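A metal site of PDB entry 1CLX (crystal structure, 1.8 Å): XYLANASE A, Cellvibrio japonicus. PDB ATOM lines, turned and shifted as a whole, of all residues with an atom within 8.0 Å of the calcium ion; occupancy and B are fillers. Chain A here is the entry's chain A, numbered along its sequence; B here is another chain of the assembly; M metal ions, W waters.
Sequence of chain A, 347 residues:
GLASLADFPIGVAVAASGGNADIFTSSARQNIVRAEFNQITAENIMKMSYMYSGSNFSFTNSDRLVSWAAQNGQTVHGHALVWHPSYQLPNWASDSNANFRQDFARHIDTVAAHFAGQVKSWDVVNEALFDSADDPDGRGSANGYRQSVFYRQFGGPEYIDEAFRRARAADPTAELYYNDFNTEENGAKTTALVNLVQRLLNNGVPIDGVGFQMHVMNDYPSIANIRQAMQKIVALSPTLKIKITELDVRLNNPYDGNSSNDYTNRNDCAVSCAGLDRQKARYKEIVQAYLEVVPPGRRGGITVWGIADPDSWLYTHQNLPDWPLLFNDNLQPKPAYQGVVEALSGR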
ATOM      1  N   LEU A 251     -10.456 -20.816 -10.005  1.00  0.00           N
ATOM      2  CA  LEU A 251     -11.776 -21.151  -9.433  1.00  0.00           C
ATOM      3  C   LEU A 251     -12.490 -22.175 -10.330  1.00  0.00           C
ATOM      4  O   LEU A 251     -13.281 -22.970  -9.823  1.00  0.00           O
ATOM      5  CB  LEU A 251     -12.652 -19.899  -9.372  1.00  0.00           C
ATOM      6  CG  LEU A 251     -12.509 -19.081  -8.107  1.00  0.00           C
ATOM      7  CD1 LEU A 251     -11.095 -18.572  -7.847  1.00  0.00           C
ATOM      8  CD2 LEU A 251     -13.553 -17.981  -8.010  1.00  0.00           C
ATOM      9  N   ASN A 252     -12.387 -22.059 -11.631  1.00  0.00           N
ATOM     10  CA  ASN A 252     -13.105 -22.917 -12.599  1.00  0.00           C
ATOM     11  C   ASN A 252     -12.336 -24.201 -12.852  1.00  0.00           C
ATOM     12  O   ASN A 252     -11.112 -24.132 -13.035  1.00  0.00           O
ATOM     13  CB  ASN A 252     -13.270 -22.169 -13.930  1.00  0.00           C
ATOM     14  CG  ASN A 252     -14.548 -21.321 -13.881  1.00  0.00           C
ATOM     15  OD1 ASN A 252     -15.585 -21.773 -13.236  1.00  0.00           O
ATOM     16  ND2 ASN A 252     -14.656 -20.142 -14.470  1.00  0.00           N
ATOM     17  N   ASN A 253     -13.011 -25.347 -12.818  1.00  0.00           N
ATOM     18  CA  ASN A 253     -12.434 -26.624 -13.319  1.00  0.00           C
ATOM     19  C   ASN A 253     -13.169 -27.149 -14.539  1.00  0.00           C
ATOM     20  O   ASN A 253     -14.296 -27.668 -14.438  1.00  0.00           O
ATOM     21  CB  ASN A 253     -12.438 -27.645 -12.161  1.00  0.00           C
ATOM     22  CG  ASN A 253     -11.768 -28.967 -12.477  1.00  0.00           C
ATOM     23  OD1 ASN A 253     -11.520 -29.396 -13.698  1.00  0.00           O
ATOM     24  ND2 ASN A 253     -11.428 -29.784 -11.480  1.00  0.00           N
ATOM     25  N   PRO A 254     -12.645 -27.029 -15.752  1.00  0.00           N
ATOM     26  CA  PRO A 254     -13.383 -27.543 -16.912  1.00  0.00           C
ATOM     27  C   PRO A 254     -13.123 -29.007 -17.218  1.00  0.00           C
ATOM     28  O   PRO A 254     -13.603 -29.495 -18.222  1.00  0.00           O
ATOM     29  CB  PRO A 254     -12.820 -26.675 -18.026  1.00  0.00           C
ATOM     30  CG  PRO A 254     -11.540 -26.050 -17.557  1.00  0.00           C
ATOM     31  CD  PRO A 254     -11.396 -26.360 -16.086  1.00  0.00           C
ATOM     32  N   TYR A 255     -12.530 -29.760 -16.310  1.00  0.00           N
ATOM     33  CA  TYR A 255     -12.093 -31.153 -16.508  1.00  0.00           C
ATOM     34  C   TYR A 255     -12.811 -32.067 -15.532  1.00  0.00           C
ATOM     35  O   TYR A 255     -12.337 -33.187 -15.311  1.00  0.00           O
ATOM     36  CB  TYR A 255     -10.597 -31.281 -16.204  1.00  0.00           C
ATOM     37  CG  TYR A 255      -9.822 -30.277 -17.056  1.00  0.00           C
ATOM     38  CD1 TYR A 255     -10.032 -30.300 -18.448  1.00  0.00           C
ATOM     39  CD2 TYR A 255      -8.956 -29.378 -16.462  1.00  0.00           C
ATOM     40  CE1 TYR A 255      -9.343 -29.388 -19.232  1.00  0.00           C
ATOM     41  CE2 TYR A 255      -8.257 -28.484 -17.261  1.00  0.00           C
ATOM     42  CZ  TYR A 255      -8.462 -28.493 -18.638  1.00  0.00           C
ATOM     43  OH  TYR A 255      -7.792 -27.598 -19.444  1.00  0.00           O
ATOM     44  N   ASP A 256     -13.838 -31.591 -14.852  1.00  0.00           N
ATOM     45  CA  ASP A 256     -14.448 -32.364 -13.758  1.00  0.00           C
ATOM     46  C   ASP A 256     -15.814 -32.931 -14.133  1.00  0.00           C
ATOM     47  O   ASP A 256     -16.539 -33.456 -13.282  1.00  0.00           O
ATOM     48  CB  ASP A 256     -14.661 -31.476 -12.531  1.00  0.00           C
ATOM     49  CG  ASP A 256     -15.511 -30.252 -12.885  1.00  0.00           C
ATOM     50  OD1 ASP A 256     -16.039 -30.083 -14.004  1.00  0.00           O
ATOM     51  OD2 ASP A 256     -15.701 -29.457 -11.955  1.00  0.00           O
ATOM     52  N   GLY A 257     -16.191 -32.797 -15.387  1.00  0.00           N
ATOM     53  CA  GLY A 257     -17.342 -33.509 -15.936  1.00  0.00           C
ATOM     54  C   GLY A 257     -18.627 -32.821 -15.511  1.00  0.00           C
ATOM     55  O   GLY A 257     -19.683 -33.421 -15.562  1.00  0.00           O
ATOM     56  N   ASN A 258     -18.506 -31.596 -15.044  1.00  0.00           N
ATOM     57  CA  ASN A 258     -19.623 -30.891 -14.415  1.00  0.00           C
ATOM     58  C   ASN A 258     -19.537 -29.431 -14.846  1.00  0.00           C
ATOM     59  O   ASN A 258     -18.728 -28.678 -14.310  1.00  0.00           O
ATOM     60  CB  ASN A 258     -19.511 -30.982 -12.889  1.00  0.00           C
ATOM     61  CG  ASN A 258     -20.683 -30.293 -12.201  1.00  0.00           C
ATOM     62  OD1 ASN A 258     -21.637 -29.702 -12.911  1.00  0.00           O
ATOM     63  ND2 ASN A 258     -20.752 -30.294 -10.878  1.00  0.00           N
ATOM     64  N   SER A 259     -20.362 -29.046 -15.805  1.00  0.00           N
ATOM     65  CA  SER A 259     -20.433 -27.664 -16.315  1.00  0.00           C
ATOM     66  C   SER A 259     -21.335 -26.836 -15.427  1.00  0.00           C
ATOM     67  O   SER A 259     -21.314 -25.610 -15.480  1.00  0.00           O
ATOM     68  CB  SER A 259     -20.878 -27.584 -17.751  1.00  0.00           C
ATOM     69  OG  SER A 259     -22.163 -28.184 -17.935  1.00  0.00           O
ATOM     70  N   SER A 260     -22.022 -27.465 -14.475  1.00  0.00           N
ATOM     71  CA  SER A 260     -22.972 -26.696 -13.658  1.00  0.00           C
ATOM     72  C   SER A 260     -22.310 -25.940 -12.523  1.00  0.00           C
ATOM     73  O   SER A 260     -22.941 -25.052 -11.935  1.00  0.00           O
ATOM     74  CB  SER A 260     -24.056 -27.619 -13.104  1.00  0.00           C
ATOM     75  OG  SER A 260     -24.837 -28.232 -14.131  1.00  0.00           O
ATOM     76  N   ASN A 261     -21.079 -26.222 -12.139  1.00  0.00           N
ATOM     77  CA  ASN A 261     -20.326 -25.531 -11.094  1.00  0.00           C
ATOM     78  C   ASN A 261     -19.317 -24.538 -11.651  1.00  0.00           C
ATOM     79  O   ASN A 261     -18.415 -24.109 -10.933  1.00  0.00           O
ATOM     80  CB  ASN A 261     -19.610 -26.546 -10.198  1.00  0.00           C
ATOM     81  CG  ASN A 261     -18.580 -27.396 -10.932  1.00  0.00           C
ATOM     82  OD1 ASN A 261     -18.269 -27.298 -12.205  1.00  0.00           O
ATOM     83  ND2 ASN A 261     -17.906 -28.320 -10.251  1.00  0.00           N
ATOM     84  N   ASP A 262     -19.449 -24.165 -12.905  1.00  0.00           N
ATOM     85  CA  ASP A 262     -18.550 -23.247 -13.585  1.00  0.00           C
ATOM     86  C   ASP A 262     -19.089 -21.821 -13.474  1.00  0.00           C
ATOM     87  O   ASP A 262     -20.290 -21.617 -13.653  1.00  0.00           O
ATOM     88  CB  ASP A 262     -18.427 -23.515 -15.077  1.00  0.00           C
ATOM     89  CG  ASP A 262     -17.816 -24.887 -15.357  1.00  0.00           C
ATOM     90  OD1 ASP A 262     -17.230 -25.435 -14.402  1.00  0.00           O
ATOM     91  OD2 ASP A 262     -17.909 -25.380 -16.493  1.00  0.00           O
ATOM     92  N   TYR A 263     -18.217 -20.866 -13.298  1.00  0.00           N
ATOM     93  CA  TYR A 263     -18.525 -19.429 -13.345  1.00  0.00           C
ATOM     94  C   TYR A 263     -18.227 -18.940 -14.772  1.00  0.00           C
ATOM     95  O   TYR A 263     -17.071 -18.949 -15.171  1.00  0.00           O
ATOM     96  CB  TYR A 263     -17.586 -18.671 -12.415  1.00  0.00           C
ATOM     97  CG  TYR A 263     -17.817 -19.010 -10.953  1.00  0.00           C
ATOM     98  CD1 TYR A 263     -18.990 -18.576 -10.333  1.00  0.00           C
ATOM     99  CD2 TYR A 263     -16.865 -19.734 -10.243  1.00  0.00           C
ATOM    100  CE1 TYR A 263     -19.204 -18.877  -8.981  1.00  0.00           C
ATOM    101  CE2 TYR A 263     -17.073 -20.039  -8.903  1.00  0.00           C
ATOM    102  CZ  TYR A 263     -18.243 -19.598  -8.276  1.00  0.00           C
ATOM    103  OH  TYR A 263     -18.459 -19.903  -6.948  1.00  0.00           O
ATOM    104  N   LEU A 320     -13.415 -19.515 -20.409  1.00  0.00           N
ATOM    105  CA  LEU A 320     -14.014 -19.256 -19.098  1.00  0.00           C
ATOM    106  C   LEU A 320     -13.244 -18.161 -18.368  1.00  0.00           C
ATOM    107  O   LEU A 320     -12.010 -18.169 -18.341  1.00  0.00           O
ATOM    108  CB  LEU A 320     -13.927 -20.516 -18.231  1.00  0.00           C
ATOM    109  CG  LEU A 320     -14.972 -21.524 -18.658  1.00  0.00           C
ATOM    110  CD1 LEU A 320     -14.662 -22.895 -18.071  1.00  0.00           C
ATOM    111  CD2 LEU A 320     -16.413 -21.120 -18.454  1.00  0.00           C
ATOM    112  N   SER B  86     -14.543 -30.005 -23.239  1.00  0.00           N
ATOM    113  CA  SER B  86     -15.134 -30.462 -21.971  1.00  0.00           C
ATOM    114  C   SER B  86     -15.794 -29.297 -21.231  1.00  0.00           C
ATOM    115  O   SER B  86     -16.832 -29.550 -20.632  1.00  0.00           O
ATOM    116  CB  SER B  86     -14.124 -31.170 -21.097  1.00  0.00           C
ATOM    117  OG  SER B  86     -13.080 -30.317 -20.621  1.00  0.00           O
ATOM    118  N   TYR B  87     -15.198 -28.119 -21.315  1.00  0.00           N
ATOM    119  CA  TYR B  87     -15.737 -26.917 -20.656  1.00  0.00           C
ATOM    120  C   TYR B  87     -17.196 -26.658 -21.024  1.00  0.00           C
ATOM    121  O   TYR B  87     -17.930 -26.166 -20.176  1.00  0.00           O
ATOM    122  CB  TYR B  87     -14.892 -25.687 -20.844  1.00  0.00           C
ATOM    123  CG  TYR B  87     -14.942 -25.076 -22.246  1.00  0.00           C
ATOM    124  CD1 TYR B  87     -15.890 -24.115 -22.592  1.00  0.00           C
ATOM    125  CD2 TYR B  87     -13.993 -25.486 -23.176  1.00  0.00           C
ATOM    126  CE1 TYR B  87     -15.889 -23.561 -23.885  1.00  0.00           C
ATOM    127  CE2 TYR B  87     -13.995 -24.941 -24.459  1.00  0.00           C
ATOM    128  CZ  TYR B  87     -14.943 -23.980 -24.805  1.00  0.00           C
ATOM    129  OH  TYR B  87     -14.902 -23.468 -26.097  1.00  0.00           O
ATOM    130  N   ASN B  91     -23.896 -31.982 -18.865  1.00  0.00           N
ATOM    131  CA  ASN B  91     -23.681 -33.079 -17.935  1.00  0.00           C
ATOM    132  C   ASN B  91     -24.000 -34.453 -18.472  1.00  0.00           C
ATOM    133  O   ASN B  91     -23.358 -35.410 -18.003  1.00  0.00           O
ATOM    134  CB  ASN B  91     -24.315 -32.815 -16.577  1.00  0.00           C
ATOM    135  CG  ASN B  91     -23.658 -31.625 -15.876  1.00  0.00           C
ATOM    136  OD1 ASN B  91     -22.460 -31.212 -16.263  1.00  0.00           O
ATOM    137  ND2 ASN B  91     -24.265 -31.029 -14.881  1.00  0.00           N
HETATM  138 CA    CA M   1     -16.665 -27.687 -13.813  1.00  0.00          CA
HETATM  139  O   HOH W   1     -16.559 -28.010 -16.301  1.00  0.00           O
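The side-chain amide oxygen (OD1) of Asn 258 is in hydrogen-bond range of the backbone NH (N) of Ser 260, at 2.8 Å.
OD1 of Asn 253 sits at hydrogen-bond distance from N of Tyr 255, at 2.8 Å.
Within 4 Å of the calcium ion: Asn 253, Asp 256, Asn 258, Asn 261 and Asp 262.
The nearest printed residue that does not touch the calcium ion is Ser 259 (4.4 Å).
OD1 of Asn 261 binds the calcium ion.
O of Asn 258 binds the calcium ion, at 2.3 Å.
The calcium ion is bound by OD1 of Asp 262, 2.4 Å away.
O of Asn 253 is bound to the calcium ion.
OD1 of Asp 256 is bound to the calcium ion, 2.5 Å away.
Water W1 is bound to the calcium ion (2.5 Å).
The side-chain carboxylate (OD2) of Asp 256 binds the calcium ion.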
